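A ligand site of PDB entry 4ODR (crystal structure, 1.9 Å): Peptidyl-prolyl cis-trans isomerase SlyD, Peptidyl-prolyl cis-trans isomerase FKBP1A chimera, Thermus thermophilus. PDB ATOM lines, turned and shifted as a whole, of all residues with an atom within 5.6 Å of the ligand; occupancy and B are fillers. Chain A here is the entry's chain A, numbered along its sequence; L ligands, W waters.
The backbone NH of Ile 11 lies within hydrogen-bond range of the backbone carbonyl oxygen of Leu 27 (2.8 Å). O of Asp 23 is in hydrogen-bond range of N of Leu 15, 2.8 Å away. The side-chain hydroxyl of Tyr 13 lies within hydrogen-bond range of the side-chain carboxylate of Asp 23. The backbone carbonyl oxygen (O) of Leu 15 is in hydrogen-bond range of the backbone NH (N) of Leu 22.
Merely in contact with the ligand: Leu 36, Tyr 13, Leu 15, Ala 62, Leu 40, Leu 27, Ile 71, Ile 72 and Phe 80. The nearest printed residue that does not touch the ligand is Ile 11 (4.5 Å).
The backbone NH (N) of Ile 37 sits at hydrogen-bond distance from an oxygen (O2) of the ligand (2.9 Å). O10 of the ligand is in hydrogen-bond range of O of Asn 35 (2.5 Å). An oxygen (O6) of the ligand sits at hydrogen-bond distance from the side-chain carboxylate of Asp 23 (2.8 Å). O3 of the ligand sits at hydrogen-bond distance from OH of Tyr 63 (2.6 Å).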
ATOM      1  N   ILE A  11     -12.730 -22.416   3.214  1.00  0.00           N
ATOM      2  CA  ILE A  11     -12.701 -23.299   4.381  1.00  0.00           C
ATOM      3  C   ILE A  11     -14.016 -23.337   5.148  1.00  0.00           C
ATOM      4  O   ILE A  11     -14.714 -22.328   5.239  1.00  0.00           O
ATOM      5  CB  ILE A  11     -11.594 -22.893   5.370  1.00  0.00           C
ATOM      6  CG1 ILE A  11     -11.760 -21.438   5.810  1.00  0.00           C
ATOM      7  CG2 ILE A  11     -10.204 -23.147   4.773  1.00  0.00           C
ATOM      8  CD1 ILE A  11     -10.841 -21.045   6.959  1.00  0.00           C
ATOM      9  N   TYR A  13     -15.138 -23.998   9.072  1.00  0.00           N
ATOM     10  CA  TYR A  13     -14.450 -23.997  10.355  1.00  0.00           C
ATOM     11  C   TYR A  13     -15.421 -24.067  11.519  1.00  0.00           C
ATOM     12  O   TYR A  13     -16.572 -23.615  11.431  1.00  0.00           O
ATOM     13  CB  TYR A  13     -13.570 -22.747  10.503  1.00  0.00           C
ATOM     14  CG  TYR A  13     -14.385 -21.475  10.671  1.00  0.00           C
ATOM     15  CD1 TYR A  13     -14.874 -20.782   9.572  1.00  0.00           C
ATOM     16  CD2 TYR A  13     -14.675 -20.972  11.938  1.00  0.00           C
ATOM     17  CE1 TYR A  13     -15.630 -19.630   9.713  1.00  0.00           C
ATOM     18  CE2 TYR A  13     -15.446 -19.813  12.096  1.00  0.00           C
ATOM     19  CZ  TYR A  13     -15.916 -19.143  10.979  1.00  0.00           C
ATOM     20  OH  TYR A  13     -16.675 -18.004  11.115  1.00  0.00           O
ATOM     21  N   LEU A  15     -14.924 -22.969  15.647  1.00  0.00           N
ATOM     22  CA  LEU A  15     -14.034 -22.379  16.629  1.00  0.00           C
ATOM     23  C   LEU A  15     -14.489 -22.712  18.045  1.00  0.00           C
ATOM     24  O   LEU A  15     -15.641 -22.450  18.408  1.00  0.00           O
ATOM     25  CB  LEU A  15     -13.960 -20.859  16.463  1.00  0.00           C
ATOM     26  CG  LEU A  15     -13.253 -20.106  17.596  1.00  0.00           C
ATOM     27  CD1 LEU A  15     -11.793 -20.554  17.742  1.00  0.00           C
ATOM     28  CD2 LEU A  15     -13.349 -18.608  17.389  1.00  0.00           C
ATOM     29  N   LEU A  22     -17.639 -21.200  19.885  1.00  0.00           N
ATOM     30  CA  LEU A  22     -17.905 -19.763  19.821  1.00  0.00           C
ATOM     31  C   LEU A  22     -18.382 -19.356  18.438  1.00  0.00           C
ATOM     32  O   LEU A  22     -19.060 -18.341  18.283  1.00  0.00           O
ATOM     33  CB  LEU A  22     -16.644 -18.970  20.179  1.00  0.00           C
ATOM     34  CG  LEU A  22     -15.983 -19.274  21.522  1.00  0.00           C
ATOM     35  CD1 LEU A  22     -14.874 -18.274  21.798  1.00  0.00           C
ATOM     36  CD2 LEU A  22     -17.006 -19.264  22.645  1.00  0.00           C
ATOM     37  N   ASP A  23     -18.018 -20.130  17.432  1.00  0.00           N
ATOM     38  CA  ASP A  23     -18.400 -19.807  16.063  1.00  0.00           C
ATOM     39  C   ASP A  23     -18.253 -21.002  15.153  1.00  0.00           C
ATOM     40  O   ASP A  23     -17.465 -21.914  15.423  1.00  0.00           O
ATOM     41  CB  ASP A  23     -17.554 -18.633  15.528  1.00  0.00           C
ATOM     42  CG  ASP A  23     -18.143 -18.002  14.280  1.00  0.00           C
ATOM     43  OD1 ASP A  23     -19.350 -18.203  14.023  1.00  0.00           O
ATOM     44  OD2 ASP A  23     -17.387 -17.322  13.559  1.00  0.00           O
ATOM     45  N   GLU A  26     -18.299 -20.786   7.173  1.00  0.00           N
ATOM     46  CA  GLU A  26     -17.558 -21.047   5.955  1.00  0.00           C
ATOM     47  C   GLU A  26     -17.134 -19.726   5.353  1.00  0.00           C
ATOM     48  O   GLU A  26     -17.875 -18.754   5.391  1.00  0.00           O
ATOM     49  CB  GLU A  26     -18.417 -21.844   4.971  1.00  0.00           C
ATOM     50  CG  GLU A  26     -17.738 -22.185   3.664  1.00  0.00           C
ATOM     51  CD  GLU A  26     -18.535 -23.195   2.860  1.00  0.00           C
ATOM     52  OE1 GLU A  26     -19.578 -23.670   3.367  1.00  0.00           O
ATOM     53  OE2 GLU A  26     -18.128 -23.536   1.732  1.00  0.00           O
ATOM     54  N   LEU A  27     -15.923 -19.677   4.802  1.00  0.00           N
ATOM     55  CA  LEU A  27     -15.461 -18.446   4.176  1.00  0.00           C
ATOM     56  C   LEU A  27     -14.401 -18.727   3.136  1.00  0.00           C
ATOM     57  O   LEU A  27     -13.743 -19.768   3.163  1.00  0.00           O
ATOM     58  CB  LEU A  27     -14.913 -17.488   5.215  1.00  0.00           C
ATOM     59  CG  LEU A  27     -13.635 -17.924   5.916  1.00  0.00           C
ATOM     60  CD1 LEU A  27     -12.426 -17.164   5.365  1.00  0.00           C
ATOM     61  CD2 LEU A  27     -13.760 -17.692   7.387  1.00  0.00           C
ATOM     62  N   ASN A  35      -5.234 -11.821   5.345  1.00  0.00           N
ATOM     63  CA  ASN A  35      -6.686 -11.949   5.495  1.00  0.00           C
ATOM     64  C   ASN A  35      -7.085 -12.567   6.840  1.00  0.00           C
ATOM     65  O   ASN A  35      -8.079 -12.175   7.437  1.00  0.00           O
ATOM     66  CB  ASN A  35      -7.280 -12.799   4.374  1.00  0.00           C
ATOM     67  CG  ASN A  35      -7.363 -12.073   3.036  1.00  0.00           C
ATOM     68  OD1 ASN A  35      -8.119 -12.487   2.164  1.00  0.00           O
ATOM     69  ND2 ASN A  35      -6.605 -10.987   2.880  1.00  0.00           N
ATOM     70  N   LEU A  36      -6.323 -13.553   7.291  1.00  0.00           N
ATOM     71  CA  LEU A  36      -6.640 -14.273   8.520  1.00  0.00           C
ATOM     72  C   LEU A  36      -5.626 -14.031   9.630  1.00  0.00           C
ATOM     73  O   LEU A  36      -4.517 -13.547   9.381  1.00  0.00           O
ATOM     74  CB  LEU A  36      -6.716 -15.790   8.252  1.00  0.00           C
ATOM     75  CG  LEU A  36      -7.505 -16.320   7.059  1.00  0.00           C
ATOM     76  CD1 LEU A  36      -7.551 -17.853   7.084  1.00  0.00           C
ATOM     77  CD2 LEU A  36      -8.900 -15.739   7.029  1.00  0.00           C
ATOM     78  N   ILE A  37      -5.988 -14.409  10.849  1.00  0.00           N
ATOM     79  CA  ILE A  37      -5.018 -14.422  11.941  1.00  0.00           C
ATOM     80  C   ILE A  37      -3.846 -15.302  11.525  1.00  0.00           C
ATOM     81  O   ILE A  37      -4.054 -16.356  10.933  1.00  0.00           O
ATOM     82  CB  ILE A  37      -5.628 -14.931  13.267  1.00  0.00           C
ATOM     83  CG1 ILE A  37      -6.342 -16.264  13.048  1.00  0.00           C
ATOM     84  CG2 ILE A  37      -6.600 -13.898  13.838  1.00  0.00           C
ATOM     85  CD1 ILE A  37      -6.709 -16.983  14.341  1.00  0.00           C
ATOM     86  N   LEU A  40      -3.568 -19.270  12.129  1.00  0.00           N
ATOM     87  CA  LEU A  40      -4.359 -20.189  11.329  1.00  0.00           C
ATOM     88  C   LEU A  40      -3.828 -20.260   9.893  1.00  0.00           C
ATOM     89  O   LEU A  40      -3.850 -21.326   9.294  1.00  0.00           O
ATOM     90  CB  LEU A  40      -5.844 -19.819  11.332  1.00  0.00           C
ATOM     91  CG  LEU A  40      -6.736 -20.890  10.692  1.00  0.00           C
ATOM     92  CD1 LEU A  40      -6.680 -22.179  11.484  1.00  0.00           C
ATOM     93  CD2 LEU A  40      -8.175 -20.432  10.566  1.00  0.00           C
ATOM     94  N   ALA A  62      -3.041 -14.975  17.464  1.00  0.00           N
ATOM     95  CA  ALA A  62      -4.445 -14.725  17.209  1.00  0.00           C
ATOM     96  C   ALA A  62      -4.844 -13.344  17.734  1.00  0.00           C
ATOM     97  O   ALA A  62      -4.364 -12.334  17.241  1.00  0.00           O
ATOM     98  CB  ALA A  62      -5.306 -15.826  17.839  1.00  0.00           C
ATOM     99  N   TYR A  63      -5.704 -13.302  18.752  1.00  0.00           N
ATOM    100  CA  TYR A  63      -6.241 -12.017  19.214  1.00  0.00           C
ATOM    101  C   TYR A  63      -5.528 -11.443  20.442  1.00  0.00           C
ATOM    102  O   TYR A  63      -5.931 -10.410  20.974  1.00  0.00           O
ATOM    103  CB  TYR A  63      -7.740 -12.148  19.476  1.00  0.00           C
ATOM    104  CG  TYR A  63      -8.486 -12.487  18.199  1.00  0.00           C
ATOM    105  CD1 TYR A  63      -8.884 -11.500  17.311  1.00  0.00           C
ATOM    106  CD2 TYR A  63      -8.732 -13.809  17.853  1.00  0.00           C
ATOM    107  CE1 TYR A  63      -9.548 -11.807  16.130  1.00  0.00           C
ATOM    108  CE2 TYR A  63      -9.390 -14.140  16.687  1.00  0.00           C
ATOM    109  CZ  TYR A  63      -9.790 -13.143  15.816  1.00  0.00           C
ATOM    110  OH  TYR A  63     -10.443 -13.485  14.657  1.00  0.00           O
ATOM    111  N   HIS A  68     -11.157 -10.333  21.373  1.00  0.00           N
ATOM    112  CA  HIS A  68     -12.155  -9.576  20.621  1.00  0.00           C
ATOM    113  C   HIS A  68     -13.413  -9.540  21.479  1.00  0.00           C
ATOM    114  O   HIS A  68     -14.205 -10.494  21.435  1.00  0.00           O
ATOM    115  CB  HIS A  68     -12.439 -10.189  19.245  1.00  0.00           C
ATOM    116  CG  HIS A  68     -13.336  -9.361  18.381  1.00  0.00           C
ATOM    117  ND1 HIS A  68     -12.991  -8.977  17.097  1.00  0.00           N
ATOM    118  CD2 HIS A  68     -14.568  -8.835  18.614  1.00  0.00           C
ATOM    119  CE1 HIS A  68     -13.967  -8.245  16.584  1.00  0.00           C
ATOM    120  NE2 HIS A  68     -14.927  -8.142  17.484  1.00  0.00           N
ATOM    121  N   ILE A  71     -16.718 -11.776  21.767  1.00  0.00           N
ATOM    122  CA  ILE A  71     -16.475 -13.076  21.140  1.00  0.00           C
ATOM    123  C   ILE A  71     -15.303 -13.845  21.768  1.00  0.00           C
ATOM    124  O   ILE A  71     -15.483 -14.936  22.298  1.00  0.00           O
ATOM    125  CB  ILE A  71     -16.157 -12.957  19.636  1.00  0.00           C
ATOM    126  CG1 ILE A  71     -17.044 -11.919  18.941  1.00  0.00           C
ATOM    127  CG2 ILE A  71     -16.288 -14.319  18.955  1.00  0.00           C
ATOM    128  CD1 ILE A  71     -16.620 -11.664  17.509  1.00  0.00           C
ATOM    129  N   ILE A  72     -14.110 -13.269  21.685  1.00  0.00           N
ATOM    130  CA  ILE A  72     -12.883 -13.937  22.120  1.00  0.00           C
ATOM    131  C   ILE A  72     -12.353 -13.275  23.380  1.00  0.00           C
ATOM    132  O   ILE A  72     -12.095 -12.072  23.377  1.00  0.00           O
ATOM    133  CB  ILE A  72     -11.787 -13.888  21.030  1.00  0.00           C
ATOM    134  CG1 ILE A  72     -12.343 -14.297  19.665  1.00  0.00           C
ATOM    135  CG2 ILE A  72     -10.573 -14.736  21.429  1.00  0.00           C
ATOM    136  CD1 ILE A  72     -12.645 -15.765  19.551  1.00  0.00           C
ATOM    137  N   LEU A  78      -7.062 -20.586  20.632  1.00  0.00           N
ATOM    138  CA  LEU A  78      -8.172 -20.907  19.756  1.00  0.00           C
ATOM    139  C   LEU A  78      -8.045 -22.314  19.202  1.00  0.00           C
ATOM    140  O   LEU A  78      -7.020 -22.655  18.591  1.00  0.00           O
ATOM    141  CB  LEU A  78      -8.263 -19.897  18.600  1.00  0.00           C
ATOM    142  CG  LEU A  78      -8.234 -18.412  18.975  1.00  0.00           C
ATOM    143  CD1 LEU A  78      -8.598 -17.570  17.769  1.00  0.00           C
ATOM    144  CD2 LEU A  78      -9.161 -18.118  20.139  1.00  0.00           C
ATOM    145  N   PHE A  80      -9.375 -24.684  16.487  1.00  0.00           N
ATOM    146  CA  PHE A  80     -10.105 -24.746  15.235  1.00  0.00           C
ATOM    147  C   PHE A  80     -10.218 -26.157  14.689  1.00  0.00           C
ATOM    148  O   PHE A  80      -9.248 -26.909  14.665  1.00  0.00           O
ATOM    149  CB  PHE A  80      -9.440 -23.878  14.170  1.00  0.00           C
ATOM    150  CG  PHE A  80      -9.641 -22.406  14.339  1.00  0.00           C
ATOM    151  CD1 PHE A  80     -10.804 -21.792  13.885  1.00  0.00           C
ATOM    152  CD2 PHE A  80      -8.642 -21.619  14.902  1.00  0.00           C
ATOM    153  CE1 PHE A  80     -10.979 -20.424  14.013  1.00  0.00           C
ATOM    154  CE2 PHE A  80      -8.817 -20.251  15.030  1.00  0.00           C
ATOM    155  CZ  PHE A  80      -9.988 -19.658  14.600  1.00  0.00           C
HETATM  156  C1  LIG L   1     -10.057 -15.007  11.084  1.00  0.00           C
HETATM  157  C2  LIG L   1     -10.386 -16.215  11.934  1.00  0.00           C
HETATM  158  C3  LIG L   1      -9.921 -17.486  11.199  1.00  0.00           C
HETATM  159  C4  LIG L   1     -10.843 -17.807  10.030  1.00  0.00           C
HETATM  160  C5  LIG L   1     -12.252 -18.054  10.547  1.00  0.00           C
HETATM  161  C6  LIG L   1     -12.740 -16.786  11.246  1.00  0.00           C
HETATM  162  C7  LIG L   1     -12.170 -16.236  13.627  1.00  0.00           C
HETATM  163  C8  LIG L   1     -13.612 -16.490  13.981  1.00  0.00           C
HETATM  164  C9  LIG L   1     -14.552 -15.284  14.032  1.00  0.00           C
HETATM  165  C10 LIG L   1     -13.872 -13.985  14.500  1.00  0.00           C
HETATM  166  C11 LIG L   1     -14.864 -12.813  14.286  1.00  0.00           C
HETATM  167  C12 LIG L   1     -15.406 -12.836  12.846  1.00  0.00           C
HETATM  168  C13 LIG L   1     -16.043 -14.217  12.583  1.00  0.00           C
HETATM  169  C14 LIG L   1     -16.596 -14.339  11.142  1.00  0.00           C
HETATM  170  C15 LIG L   1     -15.581 -13.860  10.091  1.00  0.00           C
HETATM  171  C16 LIG L   1     -15.897 -14.303   8.646  1.00  0.00           C
HETATM  172  C17 LIG L   1     -16.865 -13.284   8.011  1.00  0.00           C
HETATM  173  C18 LIG L   1     -16.124 -12.102   7.482  1.00  0.00           C
HETATM  174  C19 LIG L   1     -15.959 -11.055   8.260  1.00  0.00           C
HETATM  175  C20 LIG L   1     -15.123  -9.875   7.907  1.00  0.00           C
HETATM  176  C21 LIG L   1     -13.724 -10.061   8.486  1.00  0.00           C
HETATM  177  C22 LIG L   1     -12.743 -10.754   7.564  1.00  0.00           C
HETATM  178  C23 LIG L   1     -11.530 -11.255   8.411  1.00  0.00           C
HETATM  179  C24 LIG L   1     -11.853 -12.480   9.285  1.00  0.00           C
HETATM  180  C25 LIG L   1     -10.677 -12.883  10.222  1.00  0.00           C
HETATM  181  C26 LIG L   1     -10.407 -11.815  11.234  1.00  0.00           C
HETATM  182  C27 LIG L   1      -9.212 -11.259  11.269  1.00  0.00           C
HETATM  183  C28 LIG L   1      -8.875 -10.099  12.164  1.00  0.00           C
HETATM  184  C29 LIG L   1      -7.540 -10.389  12.867  1.00  0.00           C
HETATM  185  C30 LIG L   1      -7.183  -9.168  13.728  1.00  0.00           C
HETATM  186  C31 LIG L   1      -7.027  -7.952  12.818  1.00  0.00           C
HETATM  187  C32 LIG L   1      -8.405  -7.652  12.233  1.00  0.00           C
HETATM  188  C33 LIG L   1      -8.805  -8.822  11.336  1.00  0.00           C
HETATM  189  C34 LIG L   1     -13.545 -14.085  15.976  1.00  0.00           C
HETATM  190  C35 LIG L   1     -16.574 -15.657   8.514  1.00  0.00           C
HETATM  191  C36 LIG L   1     -15.546 -12.232   6.121  1.00  0.00           C
HETATM  192  C37 LIG L   1     -15.734  -8.643   8.577  1.00  0.00           C
HETATM  193  C38 LIG L   1     -15.228  -7.416   7.924  1.00  0.00           C
HETATM  194  C39 LIG L   1     -16.071  -6.437   7.608  1.00  0.00           C
HETATM  195  C40 LIG L   1     -12.132 -13.645   8.328  1.00  0.00           C
HETATM  196  C41 LIG L   1     -11.501 -11.495  12.200  1.00  0.00           C
HETATM  197  C42 LIG L   1     -15.779 -10.609  12.490  1.00  0.00           C
HETATM  198  C43 LIG L   1     -18.858 -14.400  11.448  1.00  0.00           C
HETATM  199  C44 LIG L   1      -6.072  -9.840  15.623  1.00  0.00           C
HETATM  200  N1  LIG L   1     -11.804 -16.384  12.333  1.00  0.00           N
HETATM  201  O1  LIG L   1     -11.029 -14.111  10.871  1.00  0.00           O
HETATM  202  O2  LIG L   1      -8.885 -14.716  10.828  1.00  0.00           O
HETATM  203  O3  LIG L   1     -11.343 -15.922  14.497  1.00  0.00           O
HETATM  204  O4  LIG L   1     -14.004 -17.595  14.201  1.00  0.00           O
HETATM  205  O5  LIG L   1     -15.055 -15.187  12.725  1.00  0.00           O
HETATM  206  O6  LIG L   1     -15.642 -15.591  14.855  1.00  0.00           O
HETATM  207  O7  LIG L   1     -16.398 -11.851  12.730  1.00  0.00           O
HETATM  208  O8  LIG L   1     -17.778 -13.577  11.030  1.00  0.00           O
HETATM  209  O9  LIG L   1     -13.437  -9.669   9.561  1.00  0.00           O
HETATM  210  O10 LIG L   1     -10.482 -11.581   7.525  1.00  0.00           O
HETATM  211  O11 LIG L   1      -5.900  -9.418  14.285  1.00  0.00           O
HETATM  212  O12 LIG L   1      -6.572  -6.918  13.650  1.00  0.00           O
HETATM  213  O   HOH W   1     -18.811 -11.090  10.454  1.00  0.00           O
HETATM  214  O   HOH W   2     -18.830 -11.705  13.652  1.00  0.00           O
HETATM  215  O   HOH W   3      -4.509  -6.770  15.208  1.00  0.00           O
HETATM  216  O   HOH W   4      -3.835 -10.647  12.990  1.00  0.00           O
HETATM  217  O   HOH W   5     -10.703 -12.073   4.696  1.00  0.00           O
